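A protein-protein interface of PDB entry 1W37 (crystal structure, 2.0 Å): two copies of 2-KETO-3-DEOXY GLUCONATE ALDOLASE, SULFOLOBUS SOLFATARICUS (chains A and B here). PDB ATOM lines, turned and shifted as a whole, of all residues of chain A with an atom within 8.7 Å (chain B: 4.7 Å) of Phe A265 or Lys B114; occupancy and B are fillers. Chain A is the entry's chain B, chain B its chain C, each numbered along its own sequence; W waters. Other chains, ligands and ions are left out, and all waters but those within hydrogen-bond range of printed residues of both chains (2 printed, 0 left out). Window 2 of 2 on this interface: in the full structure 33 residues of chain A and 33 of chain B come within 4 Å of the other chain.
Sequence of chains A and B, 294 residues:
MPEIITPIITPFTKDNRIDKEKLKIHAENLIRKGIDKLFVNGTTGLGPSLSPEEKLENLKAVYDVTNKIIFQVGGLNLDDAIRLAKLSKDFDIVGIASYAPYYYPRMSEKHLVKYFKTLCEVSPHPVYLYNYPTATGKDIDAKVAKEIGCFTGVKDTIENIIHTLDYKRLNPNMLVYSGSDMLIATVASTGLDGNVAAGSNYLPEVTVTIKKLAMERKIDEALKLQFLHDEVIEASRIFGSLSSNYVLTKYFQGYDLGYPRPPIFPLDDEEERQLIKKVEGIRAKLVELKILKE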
ATOM      1  N   LEU A  46     -24.538  10.880  34.909  1.00  0.00           N
ATOM      2  CA  LEU A  46     -23.565  10.319  33.920  1.00  0.00           C
ATOM      3  C   LEU A  46     -22.449   9.486  34.577  1.00  0.00           C
ATOM      4  O   LEU A  46     -21.294   9.502  34.168  1.00  0.00           O
ATOM      5  CB  LEU A  46     -22.975  11.450  33.084  1.00  0.00           C
ATOM      6  CG  LEU A  46     -24.043  12.279  32.360  1.00  0.00           C
ATOM      7  CD1 LEU A  46     -23.364  13.230  31.319  1.00  0.00           C
ATOM      8  CD2 LEU A  46     -25.059  11.355  31.625  1.00  0.00           C
ATOM      9  N   PHE A 239     -35.217  15.698  22.718  1.00  0.00           N
ATOM     10  CA  PHE A 239     -33.840  15.883  22.268  1.00  0.00           C
ATOM     11  C   PHE A 239     -32.821  15.024  23.012  1.00  0.00           C
ATOM     12  O   PHE A 239     -31.605  15.061  22.705  1.00  0.00           O
ATOM     13  CB  PHE A 239     -33.464  17.387  22.303  1.00  0.00           C
ATOM     14  CG  PHE A 239     -34.361  18.265  21.428  1.00  0.00           C
ATOM     15  CD1 PHE A 239     -35.201  19.230  22.006  1.00  0.00           C
ATOM     16  CD2 PHE A 239     -34.402  18.091  20.019  1.00  0.00           C
ATOM     17  CE1 PHE A 239     -36.021  20.025  21.222  1.00  0.00           C
ATOM     18  CE2 PHE A 239     -35.236  18.894  19.207  1.00  0.00           C
ATOM     19  CZ  PHE A 239     -36.052  19.844  19.795  1.00  0.00           C
ATOM     20  N   GLY A 240     -33.309  14.241  23.981  1.00  0.00           N
ATOM     21  CA  GLY A 240     -32.456  13.350  24.757  1.00  0.00           C
ATOM     22  C   GLY A 240     -32.542  13.821  26.196  1.00  0.00           C
ATOM     23  O   GLY A 240     -32.118  14.983  26.507  1.00  0.00           O
ATOM     24  N   SER A 241     -33.068  12.960  27.074  1.00  0.00           N
ATOM     25  CA  SER A 241     -33.374  13.388  28.430  1.00  0.00           C
ATOM     26  C   SER A 241     -32.149  13.824  29.215  1.00  0.00           C
ATOM     27  O   SER A 241     -32.207  14.838  29.935  1.00  0.00           O
ATOM     28  CB  SER A 241     -34.157  12.288  29.202  1.00  0.00           C
ATOM     29  OG  SER A 241     -33.242  11.238  29.541  1.00  0.00           O
ATOM     30  N   LEU A 242     -31.036  13.106  29.081  1.00  0.00           N
ATOM     31  CA  LEU A 242     -29.865  13.424  29.899  1.00  0.00           C
ATOM     32  C   LEU A 242     -29.273  14.800  29.604  1.00  0.00           C
ATOM     33  O   LEU A 242     -28.897  15.509  30.527  1.00  0.00           O
ATOM     34  CB  LEU A 242     -28.798  12.303  29.839  1.00  0.00           C
ATOM     35  CG  LEU A 242     -29.342  10.958  30.364  1.00  0.00           C
ATOM     36  CD1 LEU A 242     -28.412   9.916  29.895  1.00  0.00           C
ATOM     37  CD2 LEU A 242     -29.423  10.923  31.918  1.00  0.00           C
ATOM     38  N   SER A 243     -29.254  15.183  28.344  1.00  0.00           N
ATOM     39  CA  SER A 243     -28.923  16.544  27.942  1.00  0.00           C
ATOM     40  C   SER A 243     -30.014  17.553  28.372  1.00  0.00           C
ATOM     41  O   SER A 243     -29.733  18.674  28.860  1.00  0.00           O
ATOM     42  CB  SER A 243     -28.834  16.559  26.400  1.00  0.00           C
ATOM     43  OG  SER A 243     -27.860  15.635  25.983  1.00  0.00           O
ATOM     44  N   SER A 244     -31.265  17.192  28.113  1.00  0.00           N
ATOM     45  CA  SER A 244     -32.387  18.079  28.405  1.00  0.00           C
ATOM     46  C   SER A 244     -32.522  18.440  29.903  1.00  0.00           C
ATOM     47  O   SER A 244     -32.974  19.563  30.271  1.00  0.00           O
ATOM     48  CB  SER A 244     -33.660  17.393  27.917  1.00  0.00           C
ATOM     49  OG  SER A 244     -33.754  17.420  26.503  1.00  0.00           O
ATOM     50  N   ASN A 245     -32.168  17.493  30.769  1.00  0.00           N
ATOM     51  CA  ASN A 245     -32.217  17.706  32.238  1.00  0.00           C
ATOM     52  C   ASN A 245     -31.476  18.987  32.659  1.00  0.00           C
ATOM     53  O   ASN A 245     -31.884  19.655  33.607  1.00  0.00           O
ATOM     54  CB  ASN A 245     -31.697  16.469  33.011  1.00  0.00           C
ATOM     55  CG  ASN A 245     -32.621  15.240  32.884  1.00  0.00           C
ATOM     56  OD1 ASN A 245     -33.785  15.346  32.522  1.00  0.00           O
ATOM     57  ND2 ASN A 245     -32.083  14.067  33.190  1.00  0.00           N
ATOM     58  N   TYR A 246     -30.439  19.369  31.901  1.00  0.00           N
ATOM     59  CA  TYR A 246     -29.617  20.535  32.255  1.00  0.00           C
ATOM     60  C   TYR A 246     -30.405  21.787  31.939  1.00  0.00           C
ATOM     61  O   TYR A 246     -30.466  22.689  32.748  1.00  0.00           O
ATOM     62  CB  TYR A 246     -28.344  20.533  31.408  1.00  0.00           C
ATOM     63  CG  TYR A 246     -27.306  19.527  31.879  1.00  0.00           C
ATOM     64  CD1 TYR A 246     -27.434  18.145  31.578  1.00  0.00           C
ATOM     65  CD2 TYR A 246     -26.189  19.948  32.569  1.00  0.00           C
ATOM     66  CE1 TYR A 246     -26.521  17.230  32.014  1.00  0.00           C
ATOM     67  CE2 TYR A 246     -25.229  18.998  33.038  1.00  0.00           C
ATOM     68  CZ  TYR A 246     -25.403  17.664  32.742  1.00  0.00           C
ATOM     69  OH  TYR A 246     -24.470  16.748  33.179  1.00  0.00           O
ATOM     70  N   VAL A 247     -30.992  21.826  30.731  1.00  0.00           N
ATOM     71  CA  VAL A 247     -31.833  22.935  30.284  1.00  0.00           C
ATOM     72  C   VAL A 247     -33.085  23.094  31.190  1.00  0.00           C
ATOM     73  O   VAL A 247     -33.513  24.225  31.551  1.00  0.00           O
ATOM     74  CB  VAL A 247     -32.236  22.740  28.785  1.00  0.00           C
ATOM     75  CG1 VAL A 247     -33.423  23.659  28.372  1.00  0.00           C
ATOM     76  CG2 VAL A 247     -31.048  22.961  27.877  1.00  0.00           C
ATOM     77  N   TYR A 259     -22.451  22.065  31.535  1.00  0.00           N
ATOM     78  CA  TYR A 259     -22.601  21.260  30.318  1.00  0.00           C
ATOM     79  C   TYR A 259     -22.693  19.791  30.722  1.00  0.00           C
ATOM     80  O   TYR A 259     -22.206  19.428  31.788  1.00  0.00           O
ATOM     81  CB  TYR A 259     -21.367  21.447  29.411  1.00  0.00           C
ATOM     82  CG  TYR A 259     -21.138  22.870  28.981  1.00  0.00           C
ATOM     83  CD1 TYR A 259     -20.468  23.772  29.806  1.00  0.00           C
ATOM     84  CD2 TYR A 259     -21.610  23.319  27.728  1.00  0.00           C
ATOM     85  CE1 TYR A 259     -20.281  25.105  29.413  1.00  0.00           C
ATOM     86  CE2 TYR A 259     -21.399  24.629  27.307  1.00  0.00           C
ATOM     87  CZ  TYR A 259     -20.752  25.526  28.153  1.00  0.00           C
ATOM     88  OH  TYR A 259     -20.598  26.842  27.732  1.00  0.00           O
ATOM     89  N   PRO A 260     -23.296  18.944  29.888  1.00  0.00           N
ATOM     90  CA  PRO A 260     -23.138  17.501  30.082  1.00  0.00           C
ATOM     91  C   PRO A 260     -21.790  17.081  29.489  1.00  0.00           C
ATOM     92  O   PRO A 260     -21.025  17.943  29.004  1.00  0.00           O
ATOM     93  CB  PRO A 260     -24.305  16.896  29.307  1.00  0.00           C
ATOM     94  CG  PRO A 260     -24.802  17.950  28.372  1.00  0.00           C
ATOM     95  CD  PRO A 260     -24.173  19.265  28.752  1.00  0.00           C
ATOM     96  N   ARG A 261     -21.503  15.785  29.531  1.00  0.00           N
ATOM     97  CA  ARG A 261     -20.262  15.283  28.971  1.00  0.00           C
ATOM     98  C   ARG A 261     -20.539  14.514  27.686  1.00  0.00           C
ATOM     99  O   ARG A 261     -21.158  13.454  27.738  1.00  0.00           O
ATOM    100  CB  ARG A 261     -19.583  14.360  29.950  1.00  0.00           C
ATOM    101  CG  ARG A 261     -18.430  13.518  29.298  1.00  0.00           C
ATOM    102  CD  ARG A 261     -17.541  12.914  30.334  1.00  0.00           C
ATOM    103  NE  ARG A 261     -16.697  13.929  31.005  1.00  0.00           N
ATOM    104  CZ  ARG A 261     -15.924  13.652  32.050  1.00  0.00           C
ATOM    105  NH1 ARG A 261     -15.889  12.402  32.560  1.00  0.00           N
ATOM    106  NH2 ARG A 261     -15.149  14.598  32.559  1.00  0.00           N
ATOM    107  N   PRO A 262     -20.072  15.038  26.550  1.00  0.00           N
ATOM    108  CA  PRO A 262     -20.248  14.392  25.231  1.00  0.00           C
ATOM    109  C   PRO A 262     -19.673  12.983  25.314  1.00  0.00           C
ATOM    110  O   PRO A 262     -18.643  12.866  25.968  1.00  0.00           O
ATOM    111  CB  PRO A 262     -19.398  15.272  24.324  1.00  0.00           C
ATOM    112  CG  PRO A 262     -19.522  16.687  24.996  1.00  0.00           C
ATOM    113  CD  PRO A 262     -19.314  16.303  26.456  1.00  0.00           C
ATOM    114  N   PRO A 263     -20.265  11.949  24.725  1.00  0.00           N
ATOM    115  CA  PRO A 263     -21.402  12.027  23.778  1.00  0.00           C
ATOM    116  C   PRO A 263     -22.819  12.300  24.308  1.00  0.00           C
ATOM    117  O   PRO A 263     -23.734  12.227  23.514  1.00  0.00           O
ATOM    118  CB  PRO A 263     -21.339  10.669  23.043  1.00  0.00           C
ATOM    119  CG  PRO A 263     -20.792   9.704  24.063  1.00  0.00           C
ATOM    120  CD  PRO A 263     -19.831  10.561  24.945  1.00  0.00           C
ATOM    121  N   ILE A 264     -23.003  12.615  25.593  1.00  0.00           N
ATOM    122  CA  ILE A 264     -24.200  13.321  25.987  1.00  0.00           C
ATOM    123  C   ILE A 264     -24.070  14.797  25.623  1.00  0.00           C
ATOM    124  O   ILE A 264     -23.593  15.612  26.452  1.00  0.00           O
ATOM    125  CB  ILE A 264     -24.476  13.164  27.512  1.00  0.00           C
ATOM    126  CG1 ILE A 264     -24.325  11.700  27.925  1.00  0.00           C
ATOM    127  CG2 ILE A 264     -25.888  13.746  27.835  1.00  0.00           C
ATOM    128  CD1 ILE A 264     -25.155  10.681  27.058  1.00  0.00           C
ATOM    129  N   PHE A 265     -24.509  15.176  24.411  1.00  0.00           N
ATOM    130  CA  PHE A 265     -24.186  16.536  23.926  1.00  0.00           C
ATOM    131  C   PHE A 265     -25.161  17.567  24.480  1.00  0.00           C
ATOM    132  O   PHE A 265     -26.316  17.247  24.668  1.00  0.00           O
ATOM    133  CB  PHE A 265     -24.201  16.608  22.393  1.00  0.00           C
ATOM    134  CG  PHE A 265     -23.062  15.851  21.733  1.00  0.00           C
ATOM    135  CD1 PHE A 265     -23.278  14.579  21.209  1.00  0.00           C
ATOM    136  CD2 PHE A 265     -21.805  16.431  21.608  1.00  0.00           C
ATOM    137  CE1 PHE A 265     -22.205  13.879  20.576  1.00  0.00           C
ATOM    138  CE2 PHE A 265     -20.752  15.758  20.977  1.00  0.00           C
ATOM    139  CZ  PHE A 265     -20.975  14.475  20.470  1.00  0.00           C
ATOM    140  N   PRO A 266     -24.705  18.794  24.724  1.00  0.00           N
ATOM    141  CA  PRO A 266     -25.621  19.885  25.128  1.00  0.00           C
ATOM    142  C   PRO A 266     -26.629  20.164  24.055  1.00  0.00           C
ATOM    143  O   PRO A 266     -26.296  20.081  22.857  1.00  0.00           O
ATOM    144  CB  PRO A 266     -24.691  21.139  25.245  1.00  0.00           C
ATOM    145  CG  PRO A 266     -23.383  20.744  24.574  1.00  0.00           C
ATOM    146  CD  PRO A 266     -23.292  19.237  24.593  1.00  0.00           C
ATOM    147  N   LEU A 267     -27.863  20.475  24.438  1.00  0.00           N
ATOM    148  CA  LEU A 267     -28.811  21.015  23.456  1.00  0.00           C
ATOM    149  C   LEU A 267     -28.235  22.303  22.882  1.00  0.00           C
ATOM    150  O   LEU A 267     -27.527  23.027  23.602  1.00  0.00           O
ATOM    151  CB  LEU A 267     -30.160  21.352  24.098  1.00  0.00           C
ATOM    152  CG  LEU A 267     -31.006  20.301  24.823  1.00  0.00           C
ATOM    153  CD1 LEU A 267     -32.468  20.590  24.588  1.00  0.00           C
ATOM    154  CD2 LEU A 267     -30.684  18.830  24.475  1.00  0.00           C
ATOM    155  N   ASP A 268     -28.516  22.568  21.603  1.00  0.00           N
ATOM    156  CA  ASP A 268     -28.156  23.884  21.009  1.00  0.00           C
ATOM    157  C   ASP A 268     -29.246  24.920  21.321  1.00  0.00           C
ATOM    158  O   ASP A 268     -30.231  24.631  22.033  1.00  0.00           O
ATOM    159  CB  ASP A 268     -27.794  23.845  19.475  1.00  0.00           C
ATOM    160  CG  ASP A 268     -28.967  23.454  18.578  1.00  0.00           C
ATOM    161  OD1 ASP A 268     -30.141  23.711  18.937  1.00  0.00           O
ATOM    162  OD2 ASP A 268     -28.813  22.853  17.492  1.00  0.00           O
ATOM    163  N   GLU A 271     -32.733  24.002  20.039  1.00  0.00           N
ATOM    164  CA  GLU A 271     -33.367  22.878  20.732  1.00  0.00           C
ATOM    165  C   GLU A 271     -33.859  23.371  22.102  1.00  0.00           C
ATOM    166  O   GLU A 271     -34.990  23.066  22.515  1.00  0.00           O
ATOM    167  CB  GLU A 271     -32.374  21.699  20.867  1.00  0.00           C
ATOM    168  CG  GLU A 271     -31.946  21.144  19.489  1.00  0.00           C
ATOM    169  CD  GLU A 271     -30.753  20.200  19.527  1.00  0.00           C
ATOM    170  OE1 GLU A 271     -29.841  20.363  20.361  1.00  0.00           O
ATOM    171  OE2 GLU A 271     -30.696  19.287  18.660  1.00  0.00           O
ATOM    172  N   LEU B  78     -15.769  11.588  25.258  1.00  0.00           N
ATOM    173  CA  LEU B  78     -15.383  11.839  23.866  1.00  0.00           C
ATOM    174  C   LEU B  78     -13.978  12.408  23.764  1.00  0.00           C
ATOM    175  O   LEU B  78     -13.256  12.104  22.784  1.00  0.00           O
ATOM    176  CB  LEU B  78     -16.395  12.735  23.151  1.00  0.00           C
ATOM    177  CG  LEU B  78     -16.187  13.035  21.664  1.00  0.00           C
ATOM    178  CD1 LEU B  78     -15.779  11.780  20.802  1.00  0.00           C
ATOM    179  CD2 LEU B  78     -17.447  13.702  21.105  1.00  0.00           C
ATOM    180  N   LYS B 110     -29.195  12.037  16.062  1.00  0.00           N
ATOM    181  CA  LYS B 110     -28.280  13.174  15.864  1.00  0.00           C
ATOM    182  C   LYS B 110     -27.042  13.127  16.741  1.00  0.00           C
ATOM    183  O   LYS B 110     -25.958  13.413  16.265  1.00  0.00           O
ATOM    184  CB  LYS B 110     -28.966  14.543  16.072  1.00  0.00           C
ATOM    185  CG  LYS B 110     -29.986  14.896  14.981  1.00  0.00           C
ATOM    186  CD  LYS B 110     -30.213  16.409  15.041  1.00  0.00           C
ATOM    187  CE  LYS B 110     -31.428  16.837  14.246  1.00  0.00           C
ATOM    188  NZ  LYS B 110     -31.291  18.307  14.038  1.00  0.00           N
ATOM    189  N   HIS B 111     -27.216  12.786  18.017  1.00  0.00           N
ATOM    190  CA  HIS B 111     -26.092  12.697  18.939  1.00  0.00           C
ATOM    191  C   HIS B 111     -25.203  11.515  18.571  1.00  0.00           C
ATOM    192  O   HIS B 111     -23.984  11.645  18.655  1.00  0.00           O
ATOM    193  CB  HIS B 111     -26.572  12.566  20.405  1.00  0.00           C
ATOM    194  CG  HIS B 111     -27.128  13.836  20.989  1.00  0.00           C
ATOM    195  ND1 HIS B 111     -27.139  15.048  20.307  1.00  0.00           N
ATOM    196  CD2 HIS B 111     -27.705  14.075  22.192  1.00  0.00           C
ATOM    197  CE1 HIS B 111     -27.676  15.974  21.084  1.00  0.00           C
ATOM    198  NE2 HIS B 111     -28.040  15.404  22.223  1.00  0.00           N
ATOM    199  N   LEU B 112     -25.798  10.371  18.198  1.00  0.00           N
ATOM    200  CA  LEU B 112     -25.017   9.238  17.731  1.00  0.00           C
ATOM    201  C   LEU B 112     -24.180   9.571  16.501  1.00  0.00           C
ATOM    202  O   LEU B 112     -22.953   9.254  16.473  1.00  0.00           O
ATOM    203  CB  LEU B 112     -25.869   7.971  17.500  1.00  0.00           C
ATOM    204  CG  LEU B 112     -26.569   7.416  18.765  1.00  0.00           C
ATOM    205  CD1 LEU B 112     -27.729   6.458  18.355  1.00  0.00           C
ATOM    206  CD2 LEU B 112     -25.557   6.757  19.726  1.00  0.00           C
ATOM    207  N   VAL B 113     -24.839  10.195  15.497  1.00  0.00           N
ATOM    208  CA  VAL B 113     -24.177  10.638  14.277  1.00  0.00           C
ATOM    209  C   VAL B 113     -23.027  11.610  14.644  1.00  0.00           C
ATOM    210  O   VAL B 113     -21.883  11.416  14.200  1.00  0.00           O
ATOM    211  CB  VAL B 113     -25.177  11.228  13.244  1.00  0.00           C
ATOM    212  CG1 VAL B 113     -24.420  11.890  12.055  1.00  0.00           C
ATOM    213  CG2 VAL B 113     -26.036  10.150  12.740  1.00  0.00           C
ATOM    214  N   LYS B 114     -23.305  12.579  15.524  1.00  0.00           N
ATOM    215  CA  LYS B 114     -22.276  13.558  15.911  1.00  0.00           C
ATOM    216  C   LYS B 114     -21.109  12.885  16.641  1.00  0.00           C
ATOM    217  O   LYS B 114     -19.953  13.279  16.438  1.00  0.00           O
ATOM    218  CB  LYS B 114     -22.878  14.672  16.784  1.00  0.00           C
ATOM    219  CG  LYS B 114     -21.937  15.832  17.174  1.00  0.00           C
ATOM    220  CD  LYS B 114     -22.684  16.830  18.104  1.00  0.00           C
ATOM    221  CE  LYS B 114     -21.859  18.039  18.474  1.00  0.00           C
ATOM    222  NZ  LYS B 114     -21.421  18.782  17.271  1.00  0.00           N
ATOM    223  N   TYR B 115     -21.369  11.902  17.489  1.00  0.00           N
ATOM    224  CA  TYR B 115     -20.234  11.194  18.101  1.00  0.00           C
ATOM    225  C   TYR B 115     -19.294  10.629  17.012  1.00  0.00           C
ATOM    226  O   TYR B 115     -18.079  10.851  17.031  1.00  0.00           O
ATOM    227  CB  TYR B 115     -20.744  10.074  19.009  1.00  0.00           C
ATOM    228  CG  TYR B 115     -19.659   9.114  19.491  1.00  0.00           C
ATOM    229  CD1 TYR B 115     -18.911   9.420  20.635  1.00  0.00           C
ATOM    230  CD2 TYR B 115     -19.413   7.896  18.831  1.00  0.00           C
ATOM    231  CE1 TYR B 115     -17.913   8.543  21.119  1.00  0.00           C
ATOM    232  CE2 TYR B 115     -18.410   6.998  19.293  1.00  0.00           C
ATOM    233  CZ  TYR B 115     -17.686   7.336  20.452  1.00  0.00           C
ATOM    234  OH  TYR B 115     -16.689   6.534  20.945  1.00  0.00           O
ATOM    235  N   PHE B 116     -19.845   9.920  16.046  1.00  0.00           N
ATOM    236  CA  PHE B 116     -18.963   9.293  15.063  1.00  0.00           C
ATOM    237  C   PHE B 116     -18.320  10.282  14.112  1.00  0.00           C
ATOM    238  O   PHE B 116     -17.158  10.093  13.755  1.00  0.00           O
ATOM    239  CB  PHE B 116     -19.709   8.217  14.249  1.00  0.00           C
ATOM    240  CG  PHE B 116     -19.941   6.958  15.018  1.00  0.00           C
ATOM    241  CD1 PHE B 116     -21.205   6.652  15.512  1.00  0.00           C
ATOM    242  CD2 PHE B 116     -18.894   6.082  15.237  1.00  0.00           C
ATOM    243  CE1 PHE B 116     -21.414   5.474  16.197  1.00  0.00           C
ATOM    244  CE2 PHE B 116     -19.093   4.888  15.949  1.00  0.00           C
ATOM    245  CZ  PHE B 116     -20.318   4.584  16.411  1.00  0.00           C
ATOM    246  N   LYS B 117     -19.083  11.291  13.671  1.00  0.00           N
ATOM    247  CA  LYS B 117     -18.523  12.330  12.804  1.00  0.00           C
ATOM    248  C   LYS B 117     -17.356  13.074  13.483  1.00  0.00           C
ATOM    249  O   LYS B 117     -16.356  13.385  12.846  1.00  0.00           O
ATOM    250  CB  LYS B 117     -19.596  13.332  12.377  1.00  0.00           C
ATOM    251  CG  LYS B 117     -20.366  12.872  11.154  1.00  0.00           C
ATOM    252  CD  LYS B 117     -21.062  14.060  10.535  1.00  0.00           C
ATOM    253  CE  LYS B 117     -21.996  13.578   9.424  1.00  0.00           C
ATOM    254  NZ  LYS B 117     -22.757  14.679   8.743  1.00  0.00           N
ATOM    255  N   THR B 118     -17.507  13.331  14.773  1.00  0.00           N
ATOM    256  CA  THR B 118     -16.431  13.879  15.589  1.00  0.00           C
ATOM    257  C   THR B 118     -15.159  13.061  15.493  1.00  0.00           C
ATOM    258  O   THR B 118     -14.078  13.626  15.249  1.00  0.00           O
ATOM    259  CB  THR B 118     -16.886  14.051  17.063  1.00  0.00           C
ATOM    260  OG1 THR B 118     -18.024  14.910  17.087  1.00  0.00           O
ATOM    261  CG2 THR B 118     -15.782  14.859  17.931  1.00  0.00           C
HETATM  262  O   HOH W   1     -16.378  14.255  26.492  1.00  0.00           O
HETATM  263  O   HOH W   2     -32.424  18.864  16.770  1.00  0.00           O
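The backbone carbonyl oxygen of Pro A262 lies within hydrogen-bond range of the backbone NH of Leu B78 (3.2 Å).
O of Phe A265 sits at hydrogen-bond distance from OG of Ser A243, 2.6 Å away.
The side-chain hydroxyl (OG1) of Thr B118 sits at hydrogen-bond distance from the backbone carbonyl oxygen (O) of Lys B114 (2.6 Å).
Among the printed residues, pairs that only touch across the chains: Phe A239 with His B111, Ser A243 with His B111, Pro A263 with Tyr B115, Phe A265 with Leu B78, Phe A265 with His B111, Phe A265 with Lys B114 and Phe A265 with Tyr B115.
Of the printed residues of chain B, Pro A262 touches Leu B78.
Printed residues of chain B within 4 Å of Pro A263: Tyr B115.
Phe A265 touches just these residues of chain B: Leu B78, His B111, Lys B114 and Tyr B115.
Of chain A, only Phe A239, Ser A243 and Phe A265 come within 4 Å of His B111.
Printed residues of chain A within 4 Å of Tyr B115: Pro A263 and Phe A265.
Of the 10 printed residues of chain B, 4 touch a printed residue of chain A.
Printed residues of chain B that touch a printed residue of chain A: Leu B78, His B111, Lys B114 and Tyr B115.
Hydrophobic or aromatic side chains of chain B within 4 Å of the printed part of chain A: Leu B78, His B111 and Tyr B115.
Hydrophobic or aromatic side chains of chain A within 4 Å of the printed part of chain B: Pro A263 and Phe A265.
No position is printed for both chains.
Water W2 bridges the side-chain carboxylate (OE2) of Glu A271 (2.6 Å) and the side-chain amino group (NZ) of Lys B110 (3.0 Å).
Water W1 bridges the backbone carbonyl oxygen of Pro A262 (2.7 Å) and the backbone NH of Leu B78 (3.0 Å).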
